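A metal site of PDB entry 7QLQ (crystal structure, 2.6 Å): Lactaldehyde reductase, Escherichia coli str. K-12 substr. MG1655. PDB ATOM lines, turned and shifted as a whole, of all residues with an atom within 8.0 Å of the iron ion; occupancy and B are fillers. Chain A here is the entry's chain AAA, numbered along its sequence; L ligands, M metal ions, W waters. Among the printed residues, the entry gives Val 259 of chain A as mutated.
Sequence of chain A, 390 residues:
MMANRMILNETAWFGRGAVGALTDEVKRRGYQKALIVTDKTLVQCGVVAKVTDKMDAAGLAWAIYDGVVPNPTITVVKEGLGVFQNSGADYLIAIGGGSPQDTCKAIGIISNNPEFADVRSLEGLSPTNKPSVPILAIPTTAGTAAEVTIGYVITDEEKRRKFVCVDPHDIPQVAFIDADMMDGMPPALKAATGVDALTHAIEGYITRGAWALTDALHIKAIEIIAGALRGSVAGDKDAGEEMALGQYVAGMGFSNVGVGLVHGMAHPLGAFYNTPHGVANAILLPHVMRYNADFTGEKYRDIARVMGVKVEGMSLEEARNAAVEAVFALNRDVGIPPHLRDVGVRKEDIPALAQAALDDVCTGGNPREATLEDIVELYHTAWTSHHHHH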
ATOM      1  N   GLY A 143      -3.497  17.919   5.622  1.00  0.00           N
ATOM      2  CA  GLY A 143      -2.663  19.029   5.133  1.00  0.00           C
ATOM      3  C   GLY A 143      -3.073  19.576   3.787  1.00  0.00           C
ATOM      4  O   GLY A 143      -3.557  18.806   2.959  1.00  0.00           O
ATOM      5  N   THR A 144      -2.822  20.861   3.561  1.00  0.00           N
ATOM      6  CA  THR A 144      -3.161  21.556   2.292  1.00  0.00           C
ATOM      7  C   THR A 144      -1.900  21.638   1.438  1.00  0.00           C
ATOM      8  O   THR A 144      -2.052  21.963   0.262  1.00  0.00           O
ATOM      9  CB  THR A 144      -3.683  22.948   2.670  1.00  0.00           C
ATOM     10  OG1 THR A 144      -2.668  23.611   3.423  1.00  0.00           O
ATOM     11  CG2 THR A 144      -4.957  22.894   3.467  1.00  0.00           C
ATOM     12  N   ALA A 145      -0.738  21.393   2.013  1.00  0.00           N
ATOM     13  CA  ALA A 145       0.612  21.428   1.418  1.00  0.00           C
ATOM     14  C   ALA A 145       0.969  22.864   1.003  1.00  0.00           C
ATOM     15  O   ALA A 145       1.881  23.037   0.196  1.00  0.00           O
ATOM     16  CB  ALA A 145       0.688  20.460   0.259  1.00  0.00           C
ATOM     17  N   VAL A 153      -5.653  30.317  -2.055  1.00  0.00           N
ATOM     18  CA  VAL A 153      -7.115  30.522  -2.280  1.00  0.00           C
ATOM     19  C   VAL A 153      -7.623  31.577  -1.291  1.00  0.00           C
ATOM     20  O   VAL A 153      -7.587  31.332  -0.066  1.00  0.00           O
ATOM     21  CB  VAL A 153      -7.869  29.186  -2.180  1.00  0.00           C
ATOM     22  CG1 VAL A 153      -9.367  29.345  -2.438  1.00  0.00           C
ATOM     23  CG2 VAL A 153      -7.281  28.181  -3.133  1.00  0.00           C
ATOM     24  N   LYS A 162     -14.656  31.859  -3.926  1.00  0.00           N
ATOM     25  CA  LYS A 162     -13.201  31.674  -3.665  1.00  0.00           C
ATOM     26  C   LYS A 162     -12.475  31.674  -5.008  1.00  0.00           C
ATOM     27  O   LYS A 162     -12.979  31.037  -5.936  1.00  0.00           O
ATOM     28  CB  LYS A 162     -12.918  30.341  -2.943  1.00  0.00           C
ATOM     29  CG  LYS A 162     -13.652  30.153  -1.624  1.00  0.00           C
ATOM     30  CD  LYS A 162     -12.759  29.660  -0.490  1.00  0.00           C
ATOM     31  CE  LYS A 162     -12.438  28.189  -0.567  1.00  0.00           C
ATOM     32  NZ  LYS A 162     -11.288  27.849   0.313  1.00  0.00           N
ATOM     33  N   THR A 193      -8.587  17.587   6.954  1.00  0.00           N
ATOM     34  CA  THR A 193      -7.310  17.962   6.297  1.00  0.00           C
ATOM     35  C   THR A 193      -6.657  16.703   5.734  1.00  0.00           C
ATOM     36  O   THR A 193      -5.984  16.800   4.685  1.00  0.00           O
ATOM     37  CB  THR A 193      -6.415  18.748   7.264  1.00  0.00           C
ATOM     38  OG1 THR A 193      -6.057  17.876   8.336  1.00  0.00           O
ATOM     39  CG2 THR A 193      -7.080  19.999   7.807  1.00  0.00           C
ATOM     40  N   VAL A 195      -8.228  14.052   4.384  1.00  0.00           N
ATOM     41  CA  VAL A 195      -8.907  13.680   3.109  1.00  0.00           C
ATOM     42  C   VAL A 195      -8.725  14.805   2.085  1.00  0.00           C
ATOM     43  O   VAL A 195      -8.844  14.527   0.879  1.00  0.00           O
ATOM     44  CB  VAL A 195     -10.386  13.313   3.336  1.00  0.00           C
ATOM     45  CG1 VAL A 195     -11.076  12.931   2.041  1.00  0.00           C
ATOM     46  CG2 VAL A 195     -10.516  12.173   4.335  1.00  0.00           C
ATOM     47  N   ASP A 196      -8.420  16.031   2.516  1.00  0.00           N
ATOM     48  CA  ASP A 196      -8.009  17.111   1.594  1.00  0.00           C
ATOM     49  C   ASP A 196      -6.678  16.706   0.953  1.00  0.00           C
ATOM     50  O   ASP A 196      -6.546  16.859  -0.266  1.00  0.00           O
ATOM     51  CB  ASP A 196      -7.947  18.466   2.294  1.00  0.00           C
ATOM     52  CG  ASP A 196      -7.512  19.617   1.399  1.00  0.00           C
ATOM     53  OD1 ASP A 196      -7.962  19.683   0.220  1.00  0.00           O
ATOM     54  OD2 ASP A 196      -6.725  20.441   1.894  1.00  0.00           O
ATOM     55  N   ALA A 197      -5.731  16.182   1.738  1.00  0.00           N
ATOM     56  CA  ALA A 197      -4.429  15.675   1.260  1.00  0.00           C
ATOM     57  C   ALA A 197      -4.664  14.528   0.274  1.00  0.00           C
ATOM     58  O   ALA A 197      -3.984  14.481  -0.766  1.00  0.00           O
ATOM     59  CB  ALA A 197      -3.567  15.223   2.424  1.00  0.00           C
ATOM     60  N   THR A 199      -7.456  13.951  -1.491  1.00  0.00           N
ATOM     61  CA  THR A 199      -8.104  14.551  -2.675  1.00  0.00           C
ATOM     62  C   THR A 199      -7.023  15.139  -3.588  1.00  0.00           C
ATOM     63  O   THR A 199      -7.089  14.882  -4.796  1.00  0.00           O
ATOM     64  CB  THR A 199      -9.177  15.573  -2.279  1.00  0.00           C
ATOM     65  OG1 THR A 199     -10.172  14.915  -1.490  1.00  0.00           O
ATOM     66  CG2 THR A 199      -9.871  16.190  -3.479  1.00  0.00           C
ATOM     67  N   HIS A 200      -6.051  15.871  -3.045  1.00  0.00           N
ATOM     68  CA  HIS A 200      -4.926  16.453  -3.823  1.00  0.00           C
ATOM     69  C   HIS A 200      -4.197  15.345  -4.586  1.00  0.00           C
ATOM     70  O   HIS A 200      -3.851  15.560  -5.756  1.00  0.00           O
ATOM     71  CB  HIS A 200      -3.935  17.207  -2.936  1.00  0.00           C
ATOM     72  CG  HIS A 200      -4.498  18.421  -2.289  1.00  0.00           C
ATOM     73  ND1 HIS A 200      -4.104  18.833  -1.035  1.00  0.00           N
ATOM     74  CD2 HIS A 200      -5.440  19.298  -2.695  1.00  0.00           C
ATOM     75  CE1 HIS A 200      -4.786  19.920  -0.705  1.00  0.00           C
ATOM     76  NE2 HIS A 200      -5.610  20.221  -1.704  1.00  0.00           N
ATOM     77  N   GLU A 203      -6.778  13.456  -7.261  1.00  0.00           N
ATOM     78  CA  GLU A 203      -7.036  14.435  -8.359  1.00  0.00           C
ATOM     79  C   GLU A 203      -5.748  14.660  -9.149  1.00  0.00           C
ATOM     80  O   GLU A 203      -5.816  14.630 -10.392  1.00  0.00           O
ATOM     81  CB  GLU A 203      -7.567  15.752  -7.803  1.00  0.00           C
ATOM     82  CG  GLU A 203      -8.992  15.669  -7.283  1.00  0.00           C
ATOM     83  CD  GLU A 203      -9.819  16.912  -7.523  1.00  0.00           C
ATOM     84  OE1 GLU A 203     -10.760  16.844  -8.341  1.00  0.00           O
ATOM     85  OE2 GLU A 203      -9.525  17.960  -6.882  1.00  0.00           O
ATOM     86  N   PHE A 254       0.644  18.032  -7.179  1.00  0.00           N
ATOM     87  CA  PHE A 254      -0.605  18.681  -7.677  1.00  0.00           C
ATOM     88  C   PHE A 254      -0.344  20.156  -7.982  1.00  0.00           C
ATOM     89  O   PHE A 254      -0.926  20.689  -8.955  1.00  0.00           O
ATOM     90  CB  PHE A 254      -1.777  18.447  -6.727  1.00  0.00           C
ATOM     91  CG  PHE A 254      -1.895  19.372  -5.540  1.00  0.00           C
ATOM     92  CD1 PHE A 254      -2.505  20.600  -5.664  1.00  0.00           C
ATOM     93  CD2 PHE A 254      -1.471  18.968  -4.284  1.00  0.00           C
ATOM     94  CE1 PHE A 254      -2.664  21.429  -4.552  1.00  0.00           C
ATOM     95  CE2 PHE A 254      -1.633  19.787  -3.181  1.00  0.00           C
ATOM     96  CZ  PHE A 254      -2.216  21.023  -3.315  1.00  0.00           C
ATOM     97  N   VAL A 259      -5.398  19.696 -10.259  1.00  0.00           N
ATOM     98  CA  VAL A 259      -6.346  18.766  -9.586  1.00  0.00           C
ATOM     99  C   VAL A 259      -7.565  18.618 -10.524  1.00  0.00           C
ATOM    100  O   VAL A 259      -7.354  18.376 -11.732  1.00  0.00           O
ATOM    101  CB  VAL A 259      -6.687  19.266  -8.172  1.00  0.00           C
ATOM    102  CG1 VAL A 259      -5.589  18.911  -7.189  1.00  0.00           C
ATOM    103  CG2 VAL A 259      -6.967  20.747  -8.126  1.00  0.00           C
ATOM    104  N   HIS A 263     -12.195  19.837  -6.175  1.00  0.00           N
ATOM    105  CA  HIS A 263     -11.761  21.180  -5.709  1.00  0.00           C
ATOM    106  C   HIS A 263     -12.632  22.253  -6.386  1.00  0.00           C
ATOM    107  O   HIS A 263     -13.028  23.197  -5.687  1.00  0.00           O
ATOM    108  CB  HIS A 263     -10.251  21.379  -5.941  1.00  0.00           C
ATOM    109  CG  HIS A 263      -9.442  20.905  -4.775  1.00  0.00           C
ATOM    110  ND1 HIS A 263      -9.301  19.568  -4.468  1.00  0.00           N
ATOM    111  CD2 HIS A 263      -8.772  21.587  -3.818  1.00  0.00           C
ATOM    112  CE1 HIS A 263      -8.569  19.444  -3.377  1.00  0.00           C
ATOM    113  NE2 HIS A 263      -8.232  20.665  -2.963  1.00  0.00           N
ATOM    114  N   ALA A 266     -15.835  22.124  -4.504  1.00  0.00           N
ATOM    115  CA  ALA A 266     -15.619  22.370  -3.062  1.00  0.00           C
ATOM    116  C   ALA A 266     -15.496  23.878  -2.778  1.00  0.00           C
ATOM    117  O   ALA A 266     -15.978  24.318  -1.715  1.00  0.00           O
ATOM    118  CB  ALA A 266     -14.397  21.618  -2.586  1.00  0.00           C
ATOM    119  N   HIS A 267     -14.887  24.644  -3.689  1.00  0.00           N
ATOM    120  CA  HIS A 267     -14.614  26.097  -3.478  1.00  0.00           C
ATOM    121  C   HIS A 267     -15.904  26.882  -3.321  1.00  0.00           C
ATOM    122  O   HIS A 267     -16.026  27.665  -2.381  1.00  0.00           O
ATOM    123  CB  HIS A 267     -13.694  26.632  -4.572  1.00  0.00           C
ATOM    124  CG  HIS A 267     -12.272  26.204  -4.397  1.00  0.00           C
ATOM    125  ND1 HIS A 267     -11.361  26.247  -5.434  1.00  0.00           N
ATOM    126  CD2 HIS A 267     -11.630  25.684  -3.332  1.00  0.00           C
ATOM    127  CE1 HIS A 267     -10.201  25.789  -4.999  1.00  0.00           C
ATOM    128  NE2 HIS A 267     -10.347  25.435  -3.709  1.00  0.00           N
ATOM    129  N   HIS A 277     -12.898  23.173   3.985  1.00  0.00           N
ATOM    130  CA  HIS A 277     -12.418  22.749   2.644  1.00  0.00           C
ATOM    131  C   HIS A 277     -12.329  21.225   2.526  1.00  0.00           C
ATOM    132  O   HIS A 277     -12.733  20.669   1.485  1.00  0.00           O
ATOM    133  CB  HIS A 277     -11.095  23.470   2.369  1.00  0.00           C
ATOM    134  CG  HIS A 277     -10.405  23.012   1.147  1.00  0.00           C
ATOM    135  ND1 HIS A 277     -10.875  23.305  -0.099  1.00  0.00           N
ATOM    136  CD2 HIS A 277      -9.267  22.299   0.968  1.00  0.00           C
ATOM    137  CE1 HIS A 277     -10.065  22.788  -0.998  1.00  0.00           C
ATOM    138  NE2 HIS A 277      -9.064  22.157  -0.373  1.00  0.00           N
ATOM    139  N   GLY A 278     -11.797  20.558   3.555  1.00  0.00           N
ATOM    140  CA  GLY A 278     -11.542  19.104   3.543  1.00  0.00           C
ATOM    141  C   GLY A 278     -12.825  18.305   3.601  1.00  0.00           C
ATOM    142  O   GLY A 278     -12.865  17.218   2.981  1.00  0.00           O
ATOM    143  N   ASN A 281     -14.520  18.603   0.181  1.00  0.00           N
ATOM    144  CA  ASN A 281     -13.703  17.752  -0.721  1.00  0.00           C
ATOM    145  C   ASN A 281     -14.052  16.281  -0.483  1.00  0.00           C
ATOM    146  O   ASN A 281     -14.256  15.561  -1.471  1.00  0.00           O
ATOM    147  CB  ASN A 281     -12.194  17.952  -0.525  1.00  0.00           C
ATOM    148  CG  ASN A 281     -11.623  19.098  -1.310  1.00  0.00           C
ATOM    149  OD1 ASN A 281     -12.176  19.499  -2.337  1.00  0.00           O
ATOM    150  ND2 ASN A 281     -10.487  19.610  -0.868  1.00  0.00           N
ATOM    151  N   CYS A 362      -9.567  25.158 -11.020  1.00  0.00           N
ATOM    152  CA  CYS A 362      -9.286  23.716 -10.787  1.00  0.00           C
ATOM    153  C   CYS A 362     -10.047  22.826 -11.768  1.00  0.00           C
ATOM    154  O   CYS A 362      -9.532  21.735 -12.085  1.00  0.00           O
ATOM    155  CB  CYS A 362      -9.639  23.319  -9.366  1.00  0.00           C
ATOM    156  SG  CYS A 362      -8.682  24.238  -8.126  1.00  0.00           S
HETATM  157  N1  LIG L   1      -4.385  23.272  -1.810  1.00  0.00           N
HETATM  158  C1  LIG L   1      -5.512  24.446  -6.911  1.00  0.00           C
HETATM  159  C2  LIG L   1      -5.305  23.843  -2.572  1.00  0.00           C
HETATM  160  C3  LIG L   1      -1.399  25.616  -7.907  1.00  0.00           C
HETATM  161  O1  LIG L   1      -1.890  24.535  -7.121  1.00  0.00           O
HETATM  162  C4  LIG L   1      -4.661  24.979  -4.710  1.00  0.00           C
HETATM  163  C5  LIG L   1      -5.722  24.733  -5.570  1.00  0.00           C
HETATM  164  C6  LIG L   1      -4.223  24.414  -7.414  1.00  0.00           C
HETATM  165  C7  LIG L   1      -3.132  24.679  -6.557  1.00  0.00           C
HETATM  166  C8  LIG L   1      -3.363  24.963  -5.226  1.00  0.00           C
HETATM  167  O2  LIG L   1      -6.429  23.364  -2.745  1.00  0.00           O
HETATM  168  C9  LIG L   1      -4.891  25.179  -3.230  1.00  0.00           C
HETATM  169  O3  LIG L   1      -3.907  24.134  -8.711  1.00  0.00           O
HETATM  170  C10 LIG L   1      -4.622  24.835  -9.735  1.00  0.00           C
HETATM  171  N1  LG2 L   2      -4.668  22.488  16.512  1.00  0.00           N
HETATM  172  C1  LG2 L   2      -5.901  23.002  16.645  1.00  0.00           C
HETATM  173  N2  LG2 L   2      -6.598  23.748  15.787  1.00  0.00           N
HETATM  174  C2  LG2 L   2      -5.890  23.961  14.665  1.00  0.00           C
HETATM  175  C3  LG2 L   2      -4.626  23.507  14.389  1.00  0.00           C
HETATM  176  C4  LG2 L   2      -3.980  22.728  15.374  1.00  0.00           C
HETATM  177  N3  LG2 L   2      -2.766  22.220  15.229  1.00  0.00           N
HETATM  178  N4  LG2 L   2      -4.226  23.935  13.127  1.00  0.00           N
HETATM  179  C5  LG2 L   2      -5.247  24.627  12.673  1.00  0.00           C
HETATM  180  N5  LG2 L   2      -6.286  24.679  13.572  1.00  0.00           N
HETATM  181  C6  LG2 L   2      -7.570  25.348  13.406  1.00  0.00           C
HETATM  182  C7  LG2 L   2      -7.528  26.783  12.914  1.00  0.00           C
HETATM  183  O1  LG2 L   2      -7.214  27.685  13.953  1.00  0.00           O
HETATM  184  C8  LG2 L   2      -8.960  26.947  12.413  1.00  0.00           C
HETATM  185  O2  LG2 L   2      -9.846  27.275  13.489  1.00  0.00           O
HETATM  186  O3  LG2 L   2      -8.324  24.647  12.448  1.00  0.00           O
HETATM  187  C9  LG2 L   2      -9.265  25.560  11.820  1.00  0.00           C
HETATM  188  C10 LG2 L   2      -9.136  25.455  10.326  1.00  0.00           C
HETATM  189  O4  LG2 L   2      -7.844  25.984   9.945  1.00  0.00           O
HETATM  190  P1  LG2 L   2      -7.493  26.227   8.402  1.00  0.00           P
HETATM  191  O5  LG2 L   2      -6.189  26.937   8.322  1.00  0.00           O
HETATM  192  O6  LG2 L   2      -8.698  26.791   7.719  1.00  0.00           O
HETATM  193  O7  LG2 L   2      -7.303  24.707   7.931  1.00  0.00           O
HETATM  194  P2  LG2 L   2      -6.800  23.987   6.589  1.00  0.00           P
HETATM  195  O8  LG2 L   2      -5.368  23.610   6.765  1.00  0.00           O
HETATM  196  O9  LG2 L   2      -7.789  22.922   6.235  1.00  0.00           O
HETATM  197  O10 LG2 L   2      -6.903  25.207   5.542  1.00  0.00           O
HETATM  198  C11 LG2 L   2      -8.061  25.346   4.691  1.00  0.00           C
HETATM  199  O11 LG2 L   2      -6.685  26.241   2.944  1.00  0.00           O
HETATM  200  O12 LG2 L   2      -6.373  25.150   0.932  1.00  0.00           O
HETATM  201  C12 LG2 L   2      -7.034  26.192   1.548  1.00  0.00           C
HETATM  202  O13 LG2 L   2      -9.207  26.482   0.373  1.00  0.00           O
HETATM  203  C13 LG2 L   2      -8.549  26.006   1.532  1.00  0.00           C
HETATM  204  O14 LG2 L   2      -9.094  28.189   2.527  1.00  0.00           O
HETATM  205  C14 LG2 L   2      -8.991  26.790   2.762  1.00  0.00           C
HETATM  206  C15 LG2 L   2      -7.857  26.499   3.754  1.00  0.00           C
HETATM  207 FE    FE M   1      -7.251  21.331  -1.180  1.00  0.00          FE
HETATM  208  O   HOH W   1      -6.243  22.441   0.258  1.00  0.00           O
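A ring nitrogen (NE2) of His 200 lies close to a nitrogen (N1) of LIG L1 (3.3 Å). O2 of LIG L1 lies close to NE2 of His 263 (3.3 Å). The backbone carbonyl oxygen of Thr 144 lies within hydrogen-bond range of a nitrogen (N1) of LIG L1 (3.4 Å). O13 of LG2 L2 sits at hydrogen-bond distance from NZ of Lys 162, 2.5 Å away.
A ring nitrogen (NE2) of His 263 lies close to the side-chain amide nitrogen (ND2) of Asn 281 (3.3 Å). The backbone carbonyl oxygen of His 263 sits close to a ring nitrogen (ND1) of His 267. The side-chain carboxylate (OE2) of Glu 203 is in hydrogen-bond range of a ring nitrogen (ND1) of His 263, at 2.9 Å. The side-chain amide nitrogen of Asn 281 sits close to the backbone carbonyl oxygen of His 277, 3.4 Å away. OD1 of Asp 196 lies close to ND2 of Asn 281 (2.8 Å).
Asn 281 touches the iron ion. Within 4 Å of the iron ion: Asp 196, His 200, His 263, His 277 and Asn 281.
The iron ion is bound by NE2 of His 200 (2.0 Å), water W1 (2.1 Å), NE2 of His 263 (2.1 Å), NE2 of His 277 (2.1 Å) and OD1 of Asp 196 (2.3 Å). The iron ion has five donor atoms within binding distance. Slightly farther from the iron ion lies O2 of LIG L1 (2.7 Å).
Water W1 lies within hydrogen-bond range of OD2 of Asp 196, O12 of LG2 L2 and N1 of LIG L1.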
